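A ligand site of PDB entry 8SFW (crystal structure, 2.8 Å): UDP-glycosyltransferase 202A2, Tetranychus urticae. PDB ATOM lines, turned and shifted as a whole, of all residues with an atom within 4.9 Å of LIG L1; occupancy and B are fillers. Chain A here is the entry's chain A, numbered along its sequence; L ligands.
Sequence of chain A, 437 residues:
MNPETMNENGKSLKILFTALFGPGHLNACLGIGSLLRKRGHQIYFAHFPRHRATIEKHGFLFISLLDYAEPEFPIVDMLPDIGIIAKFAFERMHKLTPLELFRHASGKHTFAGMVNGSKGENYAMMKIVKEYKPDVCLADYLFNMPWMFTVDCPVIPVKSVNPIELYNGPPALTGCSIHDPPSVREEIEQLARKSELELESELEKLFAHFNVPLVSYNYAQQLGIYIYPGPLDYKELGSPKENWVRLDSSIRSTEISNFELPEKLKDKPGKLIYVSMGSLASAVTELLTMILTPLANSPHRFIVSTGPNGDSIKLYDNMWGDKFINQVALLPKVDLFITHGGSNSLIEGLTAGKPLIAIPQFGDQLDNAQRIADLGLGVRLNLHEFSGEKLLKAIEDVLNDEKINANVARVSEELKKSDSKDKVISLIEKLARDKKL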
ATOM      1  N   PRO A  23      14.483  21.361  34.015  1.00  0.00           N
ATOM      2  CA  PRO A  23      14.308  20.010  33.456  1.00  0.00           C
ATOM      3  C   PRO A  23      14.920  19.732  32.075  1.00  0.00           C
ATOM      4  O   PRO A  23      15.151  18.569  31.743  1.00  0.00           O
ATOM      5  CB  PRO A  23      12.782  19.845  33.397  1.00  0.00           C
ATOM      6  CG  PRO A  23      12.304  20.704  34.529  1.00  0.00           C
ATOM      7  CD  PRO A  23      13.213  21.917  34.516  1.00  0.00           C
ATOM      8  N   GLY A  24      15.166  20.787  31.272  1.00  0.00           N
ATOM      9  CA  GLY A  24      15.891  20.559  30.031  1.00  0.00           C
ATOM     10  C   GLY A  24      17.291  20.000  30.303  1.00  0.00           C
ATOM     11  O   GLY A  24      17.748  19.059  29.646  1.00  0.00           O
ATOM     12  N   ASN A  27      17.227  16.424  31.993  1.00  0.00           N
ATOM     13  CA  ASN A  27      16.803  15.342  31.106  1.00  0.00           C
ATOM     14  C   ASN A  27      17.904  14.865  30.167  1.00  0.00           C
ATOM     15  O   ASN A  27      17.971  13.685  29.841  1.00  0.00           O
ATOM     16  CB  ASN A  27      15.493  15.657  30.377  1.00  0.00           C
ATOM     17  CG  ASN A  27      14.292  15.642  31.292  1.00  0.00           C
ATOM     18  OD1 ASN A  27      14.295  15.071  32.384  1.00  0.00           O
ATOM     19  ND2 ASN A  27      13.211  16.255  30.837  1.00  0.00           N
ATOM     20  N   ARG A 252      16.018  10.242  27.553  1.00  0.00           N
ATOM     21  CA  ARG A 252      16.048   9.498  28.810  1.00  0.00           C
ATOM     22  C   ARG A 252      15.551   8.068  28.597  1.00  0.00           C
ATOM     23  O   ARG A 252      16.297   7.121  28.862  1.00  0.00           O
ATOM     24  CB  ARG A 252      15.362  10.250  29.956  1.00  0.00           C
ATOM     25  CG  ARG A 252      13.975  10.766  29.623  1.00  0.00           C
ATOM     26  CD  ARG A 252      13.472  11.914  30.489  1.00  0.00           C
ATOM     27  NE  ARG A 252      12.395  12.717  29.880  1.00  0.00           N
ATOM     28  CZ  ARG A 252      12.553  13.655  28.944  1.00  0.00           C
ATOM     29  NH1 ARG A 252      13.748  14.022  28.524  1.00  0.00           N
ATOM     30  NH2 ARG A 252      11.491  14.265  28.441  1.00  0.00           N
ATOM     31  N   TYR A 274       0.761  18.574  18.585  1.00  0.00           N
ATOM     32  CA  TYR A 274       1.209  18.795  19.939  1.00  0.00           C
ATOM     33  C   TYR A 274       1.699  20.229  20.094  1.00  0.00           C
ATOM     34  O   TYR A 274       2.469  20.736  19.267  1.00  0.00           O
ATOM     35  CB  TYR A 274       2.278  17.754  20.276  1.00  0.00           C
ATOM     36  CG  TYR A 274       2.895  17.893  21.646  1.00  0.00           C
ATOM     37  CD1 TYR A 274       2.104  18.070  22.765  1.00  0.00           C
ATOM     38  CD2 TYR A 274       4.268  17.804  21.813  1.00  0.00           C
ATOM     39  CE1 TYR A 274       2.651  18.189  24.023  1.00  0.00           C
ATOM     40  CE2 TYR A 274       4.831  17.897  23.072  1.00  0.00           C
ATOM     41  CZ  TYR A 274       4.018  18.118  24.179  1.00  0.00           C
ATOM     42  OH  TYR A 274       4.549  18.211  25.438  1.00  0.00           O
ATOM     43  N   SER A 276       3.564  22.635  22.966  1.00  0.00           N
ATOM     44  CA  SER A 276       4.266  22.777  24.226  1.00  0.00           C
ATOM     45  C   SER A 276       5.226  23.945  24.137  1.00  0.00           C
ATOM     46  O   SER A 276       6.069  24.006  23.221  1.00  0.00           O
ATOM     47  CB  SER A 276       4.993  21.524  24.587  1.00  0.00           C
ATOM     48  OG  SER A 276       5.786  21.717  25.755  1.00  0.00           O
ATOM     49  N   MET A 277       5.121  24.822  25.141  1.00  0.00           N
ATOM     50  CA  MET A 277       6.015  25.971  25.257  1.00  0.00           C
ATOM     51  C   MET A 277       7.112  25.715  26.291  1.00  0.00           C
ATOM     52  O   MET A 277       7.816  26.640  26.664  1.00  0.00           O
ATOM     53  CB  MET A 277       5.248  27.260  25.575  1.00  0.00           C
ATOM     54  CG  MET A 277       4.417  27.786  24.397  1.00  0.00           C
ATOM     55  SD  MET A 277       5.405  28.126  22.910  1.00  0.00           S
ATOM     56  CE  MET A 277       4.808  26.935  21.701  1.00  0.00           C
ATOM     57  N   GLY A 278       7.339  24.455  26.673  1.00  0.00           N
ATOM     58  CA  GLY A 278       8.520  24.085  27.430  1.00  0.00           C
ATOM     59  C   GLY A 278       8.220  23.836  28.914  1.00  0.00           C
ATOM     60  O   GLY A 278       7.059  23.839  29.341  1.00  0.00           O
ATOM     61  N   SER A 279       9.278  23.632  29.693  1.00  0.00           N
ATOM     62  CA  SER A 279       9.159  23.642  31.137  1.00  0.00           C
ATOM     63  C   SER A 279       9.172  25.072  31.701  1.00  0.00           C
ATOM     64  O   SER A 279       8.344  25.414  32.540  1.00  0.00           O
ATOM     65  CB  SER A 279      10.208  22.766  31.747  1.00  0.00           C
ATOM     66  OG  SER A 279      11.494  23.223  31.375  1.00  0.00           O
ATOM     67  N   LEU A 280      10.075  25.934  31.225  1.00  0.00           N
ATOM     68  CA  LEU A 280      10.234  27.257  31.824  1.00  0.00           C
ATOM     69  C   LEU A 280       9.096  28.184  31.387  1.00  0.00           C
ATOM     70  O   LEU A 280       8.399  28.764  32.216  1.00  0.00           O
ATOM     71  CB  LEU A 280      11.597  27.858  31.454  1.00  0.00           C
ATOM     72  CG  LEU A 280      12.833  26.968  31.659  1.00  0.00           C
ATOM     73  CD1 LEU A 280      14.063  27.612  31.029  1.00  0.00           C
ATOM     74  CD2 LEU A 280      13.036  26.671  33.133  1.00  0.00           C
ATOM     75  N   ALA A 281       8.932  28.324  30.057  1.00  0.00           N
ATOM     76  CA  ALA A 281       8.141  29.418  29.502  1.00  0.00           C
ATOM     77  C   ALA A 281       6.638  29.176  29.662  1.00  0.00           C
ATOM     78  O   ALA A 281       5.873  30.146  29.648  1.00  0.00           O
ATOM     79  CB  ALA A 281       8.523  29.686  28.061  1.00  0.00           C
ATOM     80  N   SER A 305       0.421  20.798  26.365  1.00  0.00           N
ATOM     81  CA  SER A 305       1.080  20.832  27.660  1.00  0.00           C
ATOM     82  C   SER A 305       0.784  22.188  28.276  1.00  0.00           C
ATOM     83  O   SER A 305       1.296  23.181  27.780  1.00  0.00           O
ATOM     84  CB  SER A 305       2.549  20.619  27.475  1.00  0.00           C
ATOM     85  OG  SER A 305       3.270  20.724  28.702  1.00  0.00           O
ATOM     86  N   LYS A 323      -1.289  19.603  32.720  1.00  0.00           N
ATOM     87  CA  LYS A 323      -0.144  20.347  33.224  1.00  0.00           C
ATOM     88  C   LYS A 323       1.145  19.745  32.684  1.00  0.00           C
ATOM     89  O   LYS A 323       1.989  20.434  32.141  1.00  0.00           O
ATOM     90  CB  LYS A 323      -0.101  20.216  34.736  1.00  0.00           C
ATOM     91  CG  LYS A 323      -1.089  21.115  35.429  1.00  0.00           C
ATOM     92  CD  LYS A 323      -0.889  21.156  36.903  1.00  0.00           C
ATOM     93  CE  LYS A 323      -1.727  22.300  37.433  1.00  0.00           C
ATOM     94  NZ  LYS A 323      -2.142  22.100  38.844  1.00  0.00           N
ATOM     95  N   PHE A 324       1.274  18.437  32.832  1.00  0.00           N
ATOM     96  CA  PHE A 324       2.475  17.771  32.387  1.00  0.00           C
ATOM     97  C   PHE A 324       2.067  16.587  31.526  1.00  0.00           C
ATOM     98  O   PHE A 324       1.320  15.724  31.951  1.00  0.00           O
ATOM     99  CB  PHE A 324       3.340  17.358  33.576  1.00  0.00           C
ATOM    100  CG  PHE A 324       4.722  16.956  33.171  1.00  0.00           C
ATOM    101  CD1 PHE A 324       5.690  17.926  32.894  1.00  0.00           C
ATOM    102  CD2 PHE A 324       5.044  15.606  32.957  1.00  0.00           C
ATOM    103  CE1 PHE A 324       6.955  17.550  32.466  1.00  0.00           C
ATOM    104  CE2 PHE A 324       6.315  15.228  32.550  1.00  0.00           C
ATOM    105  CZ  PHE A 324       7.261  16.206  32.313  1.00  0.00           C
ATOM    106  N   ILE A 325       2.592  16.550  30.305  1.00  0.00           N
ATOM    107  CA  ILE A 325       2.288  15.481  29.365  1.00  0.00           C
ATOM    108  C   ILE A 325       3.501  14.562  29.203  1.00  0.00           C
ATOM    109  O   ILE A 325       4.648  14.969  29.402  1.00  0.00           O
ATOM    110  CB  ILE A 325       1.828  16.151  28.068  1.00  0.00           C
ATOM    111  CG1 ILE A 325       0.389  16.600  28.261  1.00  0.00           C
ATOM    112  CG2 ILE A 325       2.025  15.287  26.832  1.00  0.00           C
ATOM    113  CD1 ILE A 325      -0.098  17.473  27.163  1.00  0.00           C
ATOM    114  N   GLN A 327       5.766  13.513  26.840  1.00  0.00           N
ATOM    115  CA  GLN A 327       6.130  14.064  25.534  1.00  0.00           C
ATOM    116  C   GLN A 327       6.734  13.010  24.601  1.00  0.00           C
ATOM    117  O   GLN A 327       6.433  12.953  23.399  1.00  0.00           O
ATOM    118  CB  GLN A 327       7.014  15.293  25.746  1.00  0.00           C
ATOM    119  CG  GLN A 327       7.507  15.907  24.455  1.00  0.00           C
ATOM    120  CD  GLN A 327       8.140  17.272  24.696  1.00  0.00           C
ATOM    121  OE1 GLN A 327       7.497  18.184  25.231  1.00  0.00           O
ATOM    122  NE2 GLN A 327       9.400  17.402  24.306  1.00  0.00           N
ATOM    123  N   VAL A 328       7.611  12.172  25.154  1.00  0.00           N
ATOM    124  CA  VAL A 328       8.316  11.154  24.382  1.00  0.00           C
ATOM    125  C   VAL A 328       7.364  10.048  23.899  1.00  0.00           C
ATOM    126  O   VAL A 328       7.535   9.555  22.757  1.00  0.00           O
ATOM    127  CB  VAL A 328       9.554  10.643  25.135  1.00  0.00           C
ATOM    128  CG1 VAL A 328      10.106   9.386  24.481  1.00  0.00           C
ATOM    129  CG2 VAL A 328      10.626  11.705  25.221  1.00  0.00           C
ATOM    130  N   HIS A 340       8.441  25.926  21.595  1.00  0.00           N
ATOM    131  CA  HIS A 340       9.215  27.109  21.910  1.00  0.00           C
ATOM    132  C   HIS A 340      10.616  27.050  21.284  1.00  0.00           C
ATOM    133  O   HIS A 340      11.258  28.093  21.215  1.00  0.00           O
ATOM    134  CB  HIS A 340       9.271  27.316  23.441  1.00  0.00           C
ATOM    135  CG  HIS A 340      10.043  26.287  24.201  1.00  0.00           C
ATOM    136  ND1 HIS A 340       9.768  24.938  24.156  1.00  0.00           N
ATOM    137  CD2 HIS A 340      11.077  26.420  25.052  1.00  0.00           C
ATOM    138  CE1 HIS A 340      10.619  24.268  24.922  1.00  0.00           C
ATOM    139  NE2 HIS A 340      11.405  25.157  25.493  1.00  0.00           N
ATOM    140  N   GLY A 342      13.140  24.732  22.418  1.00  0.00           N
ATOM    141  CA  GLY A 342      14.126  24.179  23.335  1.00  0.00           C
ATOM    142  C   GLY A 342      14.854  23.003  22.690  1.00  0.00           C
ATOM    143  O   GLY A 342      14.271  22.328  21.861  1.00  0.00           O
ATOM    144  N   SER A 343      16.115  22.768  23.071  1.00  0.00           N
ATOM    145  CA  SER A 343      16.939  21.757  22.434  1.00  0.00           C
ATOM    146  C   SER A 343      16.380  20.340  22.574  1.00  0.00           C
ATOM    147  O   SER A 343      16.320  19.564  21.616  1.00  0.00           O
ATOM    148  CB  SER A 343      18.330  21.855  22.949  1.00  0.00           C
ATOM    149  OG  SER A 343      18.945  23.036  22.462  1.00  0.00           O
ATOM    150  N   ASN A 344      15.944  20.014  23.780  1.00  0.00           N
ATOM    151  CA  ASN A 344      15.429  18.682  24.062  1.00  0.00           C
ATOM    152  C   ASN A 344      14.213  18.394  23.206  1.00  0.00           C
ATOM    153  O   ASN A 344      14.061  17.308  22.650  1.00  0.00           O
ATOM    154  CB  ASN A 344      15.016  18.603  25.528  1.00  0.00           C
ATOM    155  CG  ASN A 344      16.230  18.452  26.407  1.00  0.00           C
ATOM    156  OD1 ASN A 344      16.711  17.333  26.549  1.00  0.00           O
ATOM    157  ND2 ASN A 344      16.751  19.550  26.933  1.00  0.00           N
ATOM    158  N   SER A 345      13.325  19.393  23.148  1.00  0.00           N
ATOM    159  CA  SER A 345      12.079  19.248  22.402  1.00  0.00           C
ATOM    160  C   SER A 345      12.393  19.024  20.937  1.00  0.00           C
ATOM    161  O   SER A 345      11.759  18.183  20.298  1.00  0.00           O
ATOM    162  CB  SER A 345      11.177  20.435  22.617  1.00  0.00           C
ATOM    163  OG  SER A 345      10.675  20.443  23.936  1.00  0.00           O
ATOM    164  N   GLU A 348      13.722  15.492  20.443  1.00  0.00           N
ATOM    165  CA  GLU A 348      12.643  14.525  20.589  1.00  0.00           C
ATOM    166  C   GLU A 348      11.718  14.557  19.372  1.00  0.00           C
ATOM    167  O   GLU A 348      11.319  13.508  18.866  1.00  0.00           O
ATOM    168  CB  GLU A 348      11.889  14.771  21.892  1.00  0.00           C
ATOM    169  CG  GLU A 348      12.671  14.470  23.165  1.00  0.00           C
ATOM    170  CD  GLU A 348      12.079  15.012  24.461  1.00  0.00           C
ATOM    171  OE1 GLU A 348      10.852  15.272  24.490  1.00  0.00           O
ATOM    172  OE2 GLU A 348      12.862  15.235  25.425  1.00  0.00           O
ATOM    173  N   GLN A 365      16.906  29.257  22.297  1.00  0.00           N
ATOM    174  CA  GLN A 365      15.748  28.885  21.476  1.00  0.00           C
ATOM    175  C   GLN A 365      15.737  29.651  20.150  1.00  0.00           C
ATOM    176  O   GLN A 365      15.263  29.135  19.142  1.00  0.00           O
ATOM    177  CB  GLN A 365      14.439  29.230  22.181  1.00  0.00           C
ATOM    178  CG  GLN A 365      14.182  28.471  23.456  1.00  0.00           C
ATOM    179  CD  GLN A 365      13.185  29.229  24.287  1.00  0.00           C
ATOM    180  OE1 GLN A 365      12.469  30.062  23.779  1.00  0.00           O
ATOM    181  NE2 GLN A 365      13.145  28.937  25.572  1.00  0.00           N
HETATM  182  N1  LIG L   1       8.609  17.890  28.921  1.00  0.00           N
HETATM  183  C1  LIG L   1       7.797  16.786  29.095  1.00  0.00           C
HETATM  184  N2  LIG L   1       6.463  17.071  29.210  1.00  0.00           N
HETATM  185  C2  LIG L   1       5.873  18.317  29.184  1.00  0.00           C
HETATM  186  C3  LIG L   1       6.783  19.408  29.012  1.00  0.00           C
HETATM  187  C4  LIG L   1       8.098  19.161  28.893  1.00  0.00           C
HETATM  188  O1  LIG L   1       8.231  15.644  29.128  1.00  0.00           O
HETATM  189  O2  LIG L   1       4.652  18.408  29.301  1.00  0.00           O
HETATM  190  C5  LIG L   1      10.060  17.647  28.800  1.00  0.00           C
HETATM  191  C6  LIG L   1      10.522  17.447  27.354  1.00  0.00           C
HETATM  192  O3  LIG L   1      10.360  16.095  26.993  1.00  0.00           O
HETATM  193  C7  LIG L   1      11.989  17.863  27.454  1.00  0.00           C
HETATM  194  C8  LIG L   1      11.948  19.004  28.496  1.00  0.00           C
HETATM  195  O4  LIG L   1      10.752  18.777  29.279  1.00  0.00           O
HETATM  196  O5  LIG L   1      12.802  16.787  27.911  1.00  0.00           O
HETATM  197  C9  LIG L   1      11.928  20.394  27.925  1.00  0.00           C
HETATM  198  O6  LIG L   1      13.269  20.750  27.489  1.00  0.00           O
HETATM  199  P1  LIG L   1      13.463  21.837  26.333  1.00  0.00           P
HETATM  200  O7  LIG L   1      12.713  21.419  25.123  1.00  0.00           O
HETATM  201  O8  LIG L   1      14.918  22.138  26.194  1.00  0.00           O
HETATM  202  O9  LIG L   1      12.737  23.109  26.979  1.00  0.00           O
HETATM  203  P2  LIG L   1      13.069  24.025  28.252  1.00  0.00           P
HETATM  204  O10 LIG L   1      11.993  25.072  28.316  1.00  0.00           O
HETATM  205  O11 LIG L   1      14.426  24.599  27.993  1.00  0.00           O
HETATM  206  O12 LIG L   1      13.043  23.087  29.438  1.00  0.00           O
HETATM  207  C1  LG2 L   2      17.359  34.287  37.137  1.00  0.00           C
HETATM  208  C2  LG2 L   2      17.835  34.735  35.932  1.00  0.00           C
HETATM  209  C3  LG2 L   2      17.917  33.871  34.818  1.00  0.00           C
HETATM  210  C4  LG2 L   2      17.506  32.555  34.991  1.00  0.00           C
HETATM  211  C5  LG2 L   2      17.018  32.068  36.200  1.00  0.00           C
HETATM  212  C6  LG2 L   2      16.951  32.942  37.263  1.00  0.00           C
HETATM  213  C7  LG2 L   2      18.415  34.286  33.518  1.00  0.00           C
HETATM  214  C8  LG2 L   2      18.443  33.283  32.486  1.00  0.00           C
HETATM  215  C9  LG2 L   2      18.012  32.011  32.735  1.00  0.00           C
HETATM  216  C10 LG2 L   2      17.993  30.903  31.766  1.00  0.00           C
HETATM  217  C11 LG2 L   2      18.255  31.098  30.413  1.00  0.00           C
HETATM  218  C12 LG2 L   2      18.249  30.036  29.521  1.00  0.00           C
HETATM  219  C13 LG2 L   2      17.979  28.762  29.970  1.00  0.00           C
HETATM  220  C14 LG2 L   2      17.723  28.540  31.327  1.00  0.00           C
HETATM  221  C15 LG2 L   2      17.727  29.600  32.206  1.00  0.00           C
HETATM  222  O1  LG2 L   2      17.548  31.661  33.975  1.00  0.00           O
HETATM  223  O2  LG2 L   2      18.816  35.456  33.277  1.00  0.00           O
HETATM  224  O3  LG2 L   2      17.453  27.284  31.787  1.00  0.00           O
HETATM  225  O4  LG2 L   2      17.975  27.711  29.097  1.00  0.00           O
HETATM  226  O5  LG2 L   2      18.903  33.663  31.254  1.00  0.00           O
HETATM  227  O6  LG2 L   2      16.475  32.495  38.469  1.00  0.00           O
HETATM  228  O7  LG2 L   2      18.243  36.039  35.778  1.00  0.00           O
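The backbone NH (N) of Ser 279 sits at hydrogen-bond distance from an oxygen (O10) of LIG L1.
The side-chain hydroxyl (OG) of Ser 279 sits at hydrogen-bond distance from an oxygen (O12) of LIG L1, at 2.5 Å.
An oxygen (O7) of LIG L1 sits at hydrogen-bond distance from the backbone NH (N) of Ser 345 (2.9 Å).
OG of Ser 345 lies within hydrogen-bond range of O7 of LIG L1 (2.6 Å).
NH2 of Arg 252 sits at hydrogen-bond distance from O3 of LIG L1, 2.6 Å away.
The side-chain carboxylate (OE1) of Glu 348 lies within hydrogen-bond range of an oxygen (O3) of LIG L1, at 2.7 Å.
An oxygen (O2) of LIG L1 sits at hydrogen-bond distance from the side-chain hydroxyl of Ser 305.
N of Ile 325 sits at hydrogen-bond distance from O2 of LIG L1 (3.0 Å).
O of Ile 325 is in hydrogen-bond range of N2 of LIG L1 (2.8 Å).
NE2 of His 340 sits at hydrogen-bond distance from O9 of LIG L1.
The side-chain amide nitrogen of Asn 27 sits at hydrogen-bond distance from an oxygen (O5) of LIG L1, 3.0 Å away.
NE2 of Gln 327 is in hydrogen-bond range of O3 of LIG L1.
N of Asn 344 sits at hydrogen-bond distance from O8 of LIG L1 (3.4 Å).
The side-chain amide nitrogen of Asn 344 lies within hydrogen-bond range of an oxygen (O8) of LIG L1 (3.3 Å).
An oxygen (O8) of LIG L1 is in hydrogen-bond range of the backbone NH (N) of Ser 343.
The side-chain amide nitrogen (NE2) of Gln 327 lies within hydrogen-bond range of the side-chain hydroxyl (OG) of Ser 345, at 3.3 Å.
The guanidinium group (NH1) of Arg 252 lies within salt-bridge range of the side-chain carboxylate (OE2) of Glu 348 (3.4 Å).
The guanidinium group (NH1) of Arg 252 lies close to the side-chain amide nitrogen (ND2) of Asn 27.
The side-chain carboxylate (OE1) of Glu 348 sits at hydrogen-bond distance from the side-chain amide nitrogen (NE2) of Gln 327, at 2.6 Å.
OE1 of Gln 365 sits close to O of His 340 (3.5 Å).
The backbone carbonyl oxygen of Pro 23 sits close to the side-chain amide nitrogen of Asn 27, at 3.2 Å.
The side-chain amide oxygen (OE1) of Gln 327 lies within hydrogen-bond range of the side-chain hydroxyl (OH) of Tyr 274 (3.0 Å).
O of Gly 24 sits at hydrogen-bond distance from ND2 of Asn 344 (2.9 Å).
Gly 24 touches LIG L1 (N to O12, 3.6 Å).
Tyr 274 touches LIG L1 (OH to O2, 3.9 Å).
Gly 278 touches LIG L1 (CA to O10, 3.7 Å).
Leu 280 touches LIG L1.
CZ of Phe 324 touches C1 of LIG L1, 3.3 Å away.
CA of Gly 342 touches O7 of LIG L1 (3.6 Å).
Within 4 Å of LIG L1: Gly 24, Asn 27, Arg 252, Tyr 274, Gly 278, Ser 279, Leu 280, Ser 305, Phe 324, Ile 325, Gln 327, His 340, Gly 342, Ser 343, Asn 344, Ser 345 and Glu 348.
The nearest printed residue that does not touch LIG L1 is Ser 276 (4.1 Å).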
